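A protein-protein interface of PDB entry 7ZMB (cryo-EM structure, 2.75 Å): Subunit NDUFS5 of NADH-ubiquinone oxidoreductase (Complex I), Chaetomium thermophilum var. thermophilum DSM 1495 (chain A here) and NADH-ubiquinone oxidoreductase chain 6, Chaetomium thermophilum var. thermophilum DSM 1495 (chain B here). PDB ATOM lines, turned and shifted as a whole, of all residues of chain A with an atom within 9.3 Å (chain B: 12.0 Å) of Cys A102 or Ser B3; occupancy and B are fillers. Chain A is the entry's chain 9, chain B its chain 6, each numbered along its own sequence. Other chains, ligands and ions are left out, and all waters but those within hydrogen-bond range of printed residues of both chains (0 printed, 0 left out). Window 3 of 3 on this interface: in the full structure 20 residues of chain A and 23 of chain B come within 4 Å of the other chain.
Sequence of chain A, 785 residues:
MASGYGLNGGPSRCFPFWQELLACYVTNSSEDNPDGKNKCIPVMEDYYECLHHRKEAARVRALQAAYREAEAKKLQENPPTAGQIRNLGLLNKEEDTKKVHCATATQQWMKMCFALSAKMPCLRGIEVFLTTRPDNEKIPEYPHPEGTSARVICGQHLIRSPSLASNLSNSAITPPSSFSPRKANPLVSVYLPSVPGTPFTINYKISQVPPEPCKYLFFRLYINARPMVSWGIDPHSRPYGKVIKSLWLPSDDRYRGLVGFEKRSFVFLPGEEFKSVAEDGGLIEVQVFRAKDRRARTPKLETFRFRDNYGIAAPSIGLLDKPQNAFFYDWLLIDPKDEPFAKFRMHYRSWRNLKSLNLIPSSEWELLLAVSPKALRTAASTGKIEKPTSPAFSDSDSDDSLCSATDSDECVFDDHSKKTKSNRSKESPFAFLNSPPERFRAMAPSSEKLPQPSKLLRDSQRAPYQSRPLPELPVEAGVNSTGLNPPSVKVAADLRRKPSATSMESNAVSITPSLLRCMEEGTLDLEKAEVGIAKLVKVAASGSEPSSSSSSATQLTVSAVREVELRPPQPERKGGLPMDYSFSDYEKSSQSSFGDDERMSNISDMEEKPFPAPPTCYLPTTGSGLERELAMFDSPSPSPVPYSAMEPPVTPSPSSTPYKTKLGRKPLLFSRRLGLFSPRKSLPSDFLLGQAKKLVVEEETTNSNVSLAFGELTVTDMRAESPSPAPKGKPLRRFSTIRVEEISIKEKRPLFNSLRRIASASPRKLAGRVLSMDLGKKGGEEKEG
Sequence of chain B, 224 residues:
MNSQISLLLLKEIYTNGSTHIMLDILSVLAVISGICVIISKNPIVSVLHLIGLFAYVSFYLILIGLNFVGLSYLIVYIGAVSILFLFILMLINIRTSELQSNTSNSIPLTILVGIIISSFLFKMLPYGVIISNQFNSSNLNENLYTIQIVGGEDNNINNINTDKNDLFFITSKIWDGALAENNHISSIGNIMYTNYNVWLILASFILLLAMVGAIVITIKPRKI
Of the 18 printed residues of chain A, 4 touch a printed residue of chain B. Printed residues of chain A that touch a printed residue of chain B: Lys A74, Glu A77, Val A100 and Cys A102. Hydrophobic or aromatic side chains of chain A within 4 Å of the printed part of chain B: Val A100. Of the 6 printed residues of chain B, 3 touch a printed residue of chain A. Hydrophobic or aromatic side chains of chain B that line the printed part of chain A: Leu B8. Among the printed residues, 5 pairs touch across the chains. Among the printed residues, no Asp or Glu carboxylate lies within 4 Å of a Lys or Arg side-chain nitrogen of the other chain.
Ser B3 touches three residues of chain A. No residue of chain B comes within 4 Å of Lys A98. No residue of chain B comes within 4 Å of Lys A99. Of the printed residues of chain B, Val A100 touches Leu B8 (3.9 Å). Ala A103 touches none of the printed residues of chain B. Of chain A, only Lys A74 (3.8 Å) comes within 4 Å of Gln B4. Of the printed residues of chain B, Lys A74 touches Ser B3 (3.6 Å) and Gln B4 (3.8 Å). Printed residues of chain A within 4 Å of Leu B8: Val A100. Leu B7 touches none of the printed residues of chain A. The nearest printed residue of chain B that does not touch Glu A77 is Ile B5 (4.6 Å).
O of Ser B3 lies within hydrogen-bond range of SG of Cys A102, 3.7 Å away. The backbone NH (N) of Ser B3 is in hydrogen-bond range of the side-chain carboxylate (OE2) of Glu A77, 2.6 Å away.
Among the printed residues, pairs that only touch across the chains: Lys A74 with Ser B3 (3.6 Å), Lys A74 with Gln B4 (3.8 Å) and Val A100 with Leu B8 (3.9 Å).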
ATOM      1  N   GLU A  71     -18.873   6.284  12.335  1.00  0.00           N
ATOM      2  CA  GLU A  71     -19.629   5.545  13.337  1.00  0.00           C
ATOM      3  C   GLU A  71     -20.805   6.363  13.860  1.00  0.00           C
ATOM      4  O   GLU A  71     -21.857   5.805  14.190  1.00  0.00           O
ATOM      5  CB  GLU A  71     -18.711   5.128  14.485  1.00  0.00           C
ATOM      6  CG  GLU A  71     -17.414   4.474  14.036  1.00  0.00           C
ATOM      7  CD  GLU A  71     -17.626   3.421  12.965  1.00  0.00           C
ATOM      8  OE1 GLU A  71     -17.173   3.635  11.821  1.00  0.00           O
ATOM      9  OE2 GLU A  71     -18.252   2.383  13.265  1.00  0.00           O
ATOM     10  N   LYS A  74     -23.331   6.133  11.200  1.00  0.00           N
ATOM     11  CA  LYS A  74     -23.702   4.757  10.913  1.00  0.00           C
ATOM     12  C   LYS A  74     -24.901   4.324  11.747  1.00  0.00           C
ATOM     13  O   LYS A  74     -25.104   4.782  12.875  1.00  0.00           O
ATOM     14  CB  LYS A  74     -22.521   3.825  11.176  1.00  0.00           C
ATOM     15  CG  LYS A  74     -22.652   2.452  10.536  1.00  0.00           C
ATOM     16  CD  LYS A  74     -21.388   1.635  10.734  1.00  0.00           C
ATOM     17  CE  LYS A  74     -21.482   0.290  10.034  1.00  0.00           C
ATOM     18  NZ  LYS A  74     -20.237  -0.508  10.209  1.00  0.00           N
ATOM     19  N   LEU A  75     -25.706   3.436  11.168  1.00  0.00           N
ATOM     20  CA  LEU A  75     -26.866   2.906  11.868  1.00  0.00           C
ATOM     21  C   LEU A  75     -26.430   2.155  13.120  1.00  0.00           C
ATOM     22  O   LEU A  75     -25.438   1.421  13.112  1.00  0.00           O
ATOM     23  CB  LEU A  75     -27.661   1.980  10.948  1.00  0.00           C
ATOM     24  CG  LEU A  75     -28.296   2.635   9.719  1.00  0.00           C
ATOM     25  CD1 LEU A  75     -28.933   1.589   8.818  1.00  0.00           C
ATOM     26  CD2 LEU A  75     -29.312   3.688  10.133  1.00  0.00           C
ATOM     27  N   GLN A  76     -27.175   2.349  14.202  1.00  0.00           N
ATOM     28  CA  GLN A  76     -26.879   1.728  15.484  1.00  0.00           C
ATOM     29  C   GLN A  76     -27.991   0.748  15.827  1.00  0.00           C
ATOM     30  O   GLN A  76     -29.175   1.086  15.721  1.00  0.00           O
ATOM     31  CB  GLN A  76     -26.735   2.785  16.581  1.00  0.00           C
ATOM     32  CG  GLN A  76     -26.041   2.285  17.831  1.00  0.00           C
ATOM     33  CD  GLN A  76     -26.971   1.526  18.750  1.00  0.00           C
ATOM     34  OE1 GLN A  76     -28.165   1.812  18.823  1.00  0.00           O
ATOM     35  NE2 GLN A  76     -26.428   0.539  19.446  1.00  0.00           N
ATOM     36  N   GLU A  77     -27.613  -0.462  16.235  1.00  0.00           N
ATOM     37  CA  GLU A  77     -28.581  -1.510  16.540  1.00  0.00           C
ATOM     38  C   GLU A  77     -28.626  -1.869  18.022  1.00  0.00           C
ATOM     39  O   GLU A  77     -29.698  -1.820  18.632  1.00  0.00           O
ATOM     40  CB  GLU A  77     -28.290  -2.756  15.685  1.00  0.00           C
ATOM     41  CG  GLU A  77     -26.897  -3.364  15.840  1.00  0.00           C
ATOM     42  CD  GLU A  77     -25.854  -2.690  14.966  1.00  0.00           C
ATOM     43  OE1 GLU A  77     -26.086  -1.542  14.531  1.00  0.00           O
ATOM     44  OE2 GLU A  77     -24.801  -3.311  14.712  1.00  0.00           O
ATOM     45  N   ASN A  78     -27.487  -2.213  18.623  1.00  0.00           N
ATOM     46  CA  ASN A  78     -27.425  -2.598  20.028  1.00  0.00           C
ATOM     47  C   ASN A  78     -26.013  -2.391  20.561  1.00  0.00           C
ATOM     48  O   ASN A  78     -25.055  -2.954  20.017  1.00  0.00           O
ATOM     49  CB  ASN A  78     -27.854  -4.054  20.213  1.00  0.00           C
ATOM     50  CG  ASN A  78     -29.351  -4.203  20.395  1.00  0.00           C
ATOM     51  OD1 ASN A  78     -29.964  -3.496  21.191  1.00  0.00           O
ATOM     52  ND2 ASN A  78     -29.947  -5.127  19.651  1.00  0.00           N
ATOM     53  N   PRO A  80     -22.877  -3.045  22.814  1.00  0.00           N
ATOM     54  CA  PRO A  80     -22.343  -4.042  23.750  1.00  0.00           C
ATOM     55  C   PRO A  80     -21.889  -3.387  25.042  1.00  0.00           C
ATOM     56  O   PRO A  80     -20.965  -2.568  25.032  1.00  0.00           O
ATOM     57  CB  PRO A  80     -21.168  -4.662  22.978  1.00  0.00           C
ATOM     58  CG  PRO A  80     -21.317  -4.173  21.554  1.00  0.00           C
ATOM     59  CD  PRO A  80     -21.989  -2.849  21.661  1.00  0.00           C
ATOM     60  N   LEU A  88     -15.620 -11.020  27.349  1.00  0.00           N
ATOM     61  CA  LEU A  88     -15.006 -11.555  26.146  1.00  0.00           C
ATOM     62  C   LEU A  88     -13.938 -12.585  26.487  1.00  0.00           C
ATOM     63  O   LEU A  88     -13.062 -12.340  27.322  1.00  0.00           O
ATOM     64  CB  LEU A  88     -14.394 -10.423  25.331  1.00  0.00           C
ATOM     65  CG  LEU A  88     -13.881 -10.826  23.954  1.00  0.00           C
ATOM     66  CD1 LEU A  88     -15.042 -11.036  23.013  1.00  0.00           C
ATOM     67  CD2 LEU A  88     -12.952  -9.764  23.418  1.00  0.00           C
ATOM     68  N   GLU A  94     -20.068 -17.935  26.799  1.00  0.00           N
ATOM     69  CA  GLU A  94     -20.088 -17.992  25.341  1.00  0.00           C
ATOM     70  C   GLU A  94     -21.110 -17.032  24.748  1.00  0.00           C
ATOM     71  O   GLU A  94     -20.856 -16.429  23.699  1.00  0.00           O
ATOM     72  CB  GLU A  94     -20.379 -19.417  24.872  1.00  0.00           C
ATOM     73  CG  GLU A  94     -19.181 -20.347  24.919  1.00  0.00           C
ATOM     74  CD  GLU A  94     -19.120 -21.152  26.201  1.00  0.00           C
ATOM     75  OE1 GLU A  94     -19.809 -20.775  27.173  1.00  0.00           O
ATOM     76  OE2 GLU A  94     -18.387 -22.161  26.239  1.00  0.00           O
ATOM     77  N   GLU A  95     -22.266 -16.881  25.397  1.00  0.00           N
ATOM     78  CA  GLU A  95     -23.302 -16.001  24.866  1.00  0.00           C
ATOM     79  C   GLU A  95     -22.820 -14.558  24.788  1.00  0.00           C
ATOM     80  O   GLU A  95     -23.074 -13.864  23.797  1.00  0.00           O
ATOM     81  CB  GLU A  95     -24.563 -16.098  25.724  1.00  0.00           C
ATOM     82  CG  GLU A  95     -25.009 -17.519  26.009  1.00  0.00           C
ATOM     83  CD  GLU A  95     -25.627 -18.188  24.797  1.00  0.00           C
ATOM     84  OE1 GLU A  95     -26.133 -17.464  23.912  1.00  0.00           O
ATOM     85  OE2 GLU A  95     -25.606 -19.434  24.730  1.00  0.00           O
ATOM     86  N   ASP A  96     -22.125 -14.089  25.826  1.00  0.00           N
ATOM     87  CA  ASP A  96     -21.663 -12.706  25.841  1.00  0.00           C
ATOM     88  C   ASP A  96     -20.642 -12.443  24.744  1.00  0.00           C
ATOM     89  O   ASP A  96     -20.692 -11.401  24.082  1.00  0.00           O
ATOM     90  CB  ASP A  96     -21.081 -12.364  27.211  1.00  0.00           C
ATOM     91  CG  ASP A  96     -22.132 -11.868  28.181  1.00  0.00           C
ATOM     92  OD1 ASP A  96     -23.110 -11.239  27.727  1.00  0.00           O
ATOM     93  OD2 ASP A  96     -21.980 -12.107  29.397  1.00  0.00           O
ATOM     94  N   THR A  97     -19.703 -13.370  24.541  1.00  0.00           N
ATOM     95  CA  THR A  97     -18.678 -13.175  23.521  1.00  0.00           C
ATOM     96  C   THR A  97     -19.283 -13.114  22.127  1.00  0.00           C
ATOM     97  O   THR A  97     -18.878 -12.284  21.304  1.00  0.00           O
ATOM     98  CB  THR A  97     -17.631 -14.284  23.611  1.00  0.00           C
ATOM     99  OG1 THR A  97     -16.911 -14.165  24.844  1.00  0.00           O
ATOM    100  CG2 THR A  97     -16.652 -14.213  22.448  1.00  0.00           C
ATOM    101  N   LYS A  98     -20.259 -13.978  21.844  1.00  0.00           N
ATOM    102  CA  LYS A  98     -20.886 -13.978  20.526  1.00  0.00           C
ATOM    103  C   LYS A  98     -21.580 -12.651  20.251  1.00  0.00           C
ATOM    104  O   LYS A  98     -21.523 -12.126  19.133  1.00  0.00           O
ATOM    105  CB  LYS A  98     -21.871 -15.140  20.410  1.00  0.00           C
ATOM    106  CG  LYS A  98     -21.224 -16.511  20.511  1.00  0.00           C
ATOM    107  CD  LYS A  98     -22.182 -17.606  20.076  1.00  0.00           C
ATOM    108  CE  LYS A  98     -22.470 -17.527  18.587  1.00  0.00           C
ATOM    109  NZ  LYS A  98     -21.240 -17.741  17.776  1.00  0.00           N
ATOM    110  N   LYS A  99     -22.246 -12.093  21.263  1.00  0.00           N
ATOM    111  CA  LYS A  99     -22.879 -10.792  21.094  1.00  0.00           C
ATOM    112  C   LYS A  99     -21.845  -9.708  20.822  1.00  0.00           C
ATOM    113  O   LYS A  99     -22.059  -8.830  19.978  1.00  0.00           O
ATOM    114  CB  LYS A  99     -23.708 -10.453  22.332  1.00  0.00           C
ATOM    115  CG  LYS A  99     -24.037  -8.978  22.479  1.00  0.00           C
ATOM    116  CD  LYS A  99     -25.019  -8.528  21.412  1.00  0.00           C
ATOM    117  CE  LYS A  99     -25.119  -7.015  21.367  1.00  0.00           C
ATOM    118  NZ  LYS A  99     -23.800  -6.385  21.086  1.00  0.00           N
ATOM    119  N   VAL A 100     -20.712  -9.752  21.527  1.00  0.00           N
ATOM    120  CA  VAL A 100     -19.679  -8.734  21.348  1.00  0.00           C
ATOM    121  C   VAL A 100     -19.087  -8.803  19.948  1.00  0.00           C
ATOM    122  O   VAL A 100     -18.904  -7.775  19.284  1.00  0.00           O
ATOM    123  CB  VAL A 100     -18.592  -8.880  22.429  1.00  0.00           C
ATOM    124  CG1 VAL A 100     -17.425  -7.962  22.129  1.00  0.00           C
ATOM    125  CG2 VAL A 100     -19.167  -8.573  23.797  1.00  0.00           C
ATOM    126  N   HIS A 101     -18.785 -10.006  19.472  1.00  0.00           N
ATOM    127  CA  HIS A 101     -18.188 -10.153  18.152  1.00  0.00           C
ATOM    128  C   HIS A 101     -19.215 -10.188  17.029  1.00  0.00           C
ATOM    129  O   HIS A 101     -18.820 -10.232  15.859  1.00  0.00           O
ATOM    130  CB  HIS A 101     -17.334 -11.419  18.100  1.00  0.00           C
ATOM    131  CG  HIS A 101     -16.016 -11.278  18.789  1.00  0.00           C
ATOM    132  ND1 HIS A 101     -15.410 -10.058  18.984  1.00  0.00           N
ATOM    133  CD2 HIS A 101     -15.184 -12.202  19.323  1.00  0.00           C
ATOM    134  CE1 HIS A 101     -14.262 -10.235  19.613  1.00  0.00           C
ATOM    135  NE2 HIS A 101     -14.100 -11.527  19.830  1.00  0.00           N
ATOM    136  N   CYS A 102     -20.509 -10.185  17.349  1.00  0.00           N
ATOM    137  CA  CYS A 102     -21.609 -10.183  16.389  1.00  0.00           C
ATOM    138  C   CYS A 102     -21.615 -11.431  15.511  1.00  0.00           C
ATOM    139  O   CYS A 102     -22.336 -11.473  14.507  1.00  0.00           O
ATOM    140  CB  CYS A 102     -21.587  -8.922  15.513  1.00  0.00           C
ATOM    141  SG  CYS A 102     -23.104  -8.574  14.585  1.00  0.00           S
ATOM    142  N   ALA A 103     -20.842 -12.452  15.863  1.00  0.00           N
ATOM    143  CA  ALA A 103     -20.791 -13.679  15.079  1.00  0.00           C
ATOM    144  C   ALA A 103     -22.008 -14.557  15.357  1.00  0.00           C
ATOM    145  O   ALA A 103     -22.929 -14.154  16.068  1.00  0.00           O
ATOM    146  CB  ALA A 103     -19.508 -14.440  15.369  1.00  0.00           C
ATOM    147  N   SER B   3     -23.776  -2.820  12.369  1.00  0.00           N
ATOM    148  CA  SER B   3     -23.102  -3.803  11.532  1.00  0.00           C
ATOM    149  C   SER B   3     -21.897  -4.399  12.250  1.00  0.00           C
ATOM    150  O   SER B   3     -21.983  -5.477  12.837  1.00  0.00           O
ATOM    151  CB  SER B   3     -22.667  -3.175  10.208  1.00  0.00           C
ATOM    152  N   GLN B   4     -20.775  -3.689  12.197  1.00  0.00           N
ATOM    153  CA  GLN B   4     -19.536  -4.115  12.831  1.00  0.00           C
ATOM    154  C   GLN B   4     -19.096  -3.056  13.831  1.00  0.00           C
ATOM    155  O   GLN B   4     -19.029  -1.869  13.494  1.00  0.00           O
ATOM    156  CB  GLN B   4     -18.438  -4.355  11.789  1.00  0.00           C
ATOM    157  N   ILE B   5     -18.800  -3.485  15.058  1.00  0.00           N
ATOM    158  CA  ILE B   5     -18.359  -2.541  16.082  1.00  0.00           C
ATOM    159  C   ILE B   5     -16.897  -2.179  15.862  1.00  0.00           C
ATOM    160  O   ILE B   5     -16.556  -1.018  15.601  1.00  0.00           O
ATOM    161  CB  ILE B   5     -18.585  -3.130  17.482  1.00  0.00           C
ATOM    162  CG1 ILE B   5     -19.987  -3.735  17.585  1.00  0.00           C
ATOM    163  CG2 ILE B   5     -18.427  -2.046  18.521  1.00  0.00           C
ATOM    164  CD1 ILE B   5     -21.100  -2.739  17.381  1.00  0.00           C
ATOM    165  N   SER B   6     -16.015  -3.169  15.997  1.00  0.00           N
ATOM    166  CA  SER B   6     -14.626  -3.146  15.525  1.00  0.00           C
ATOM    167  C   SER B   6     -13.745  -2.311  16.449  1.00  0.00           C
ATOM    168  O   SER B   6     -12.514  -2.375  16.298  1.00  0.00           O
ATOM    169  CB  SER B   6     -14.634  -2.721  14.056  1.00  0.00           C
ATOM    170  OG  SER B   6     -15.484  -3.556  13.287  1.00  0.00           O
ATOM    171  N   LEU B   7     -14.301  -1.503  17.358  1.00  0.00           N
ATOM    172  CA  LEU B   7     -13.396  -0.785  18.305  1.00  0.00           C
ATOM    173  C   LEU B   7     -14.095  -0.633  19.646  1.00  0.00           C
ATOM    174  O   LEU B   7     -15.170  -0.011  19.672  1.00  0.00           O
ATOM    175  CB  LEU B   7     -12.929   0.576  17.772  1.00  0.00           C
ATOM    176  CG  LEU B   7     -11.634   0.595  16.952  1.00  0.00           C
ATOM    177  CD1 LEU B   7     -11.228   2.026  16.633  1.00  0.00           C
ATOM    178  CD2 LEU B   7     -10.504  -0.114  17.677  1.00  0.00           C
ATOM    179  N   LEU B   8     -13.483  -1.159  20.707  1.00  0.00           N
ATOM    180  CA  LEU B   8     -14.168  -1.161  22.018  1.00  0.00           C
ATOM    181  C   LEU B   8     -13.436  -0.269  23.005  1.00  0.00           C
ATOM    182  O   LEU B   8     -12.272  -0.568  23.319  1.00  0.00           O
ATOM    183  CB  LEU B   8     -14.210  -2.605  22.515  1.00  0.00           C
ATOM    184  CG  LEU B   8     -14.982  -3.556  21.600  1.00  0.00           C
ATOM    185  CD1 LEU B   8     -14.974  -4.971  22.143  1.00  0.00           C
ATOM    186  CD2 LEU B   8     -16.403  -3.066  21.395  1.00  0.00           C
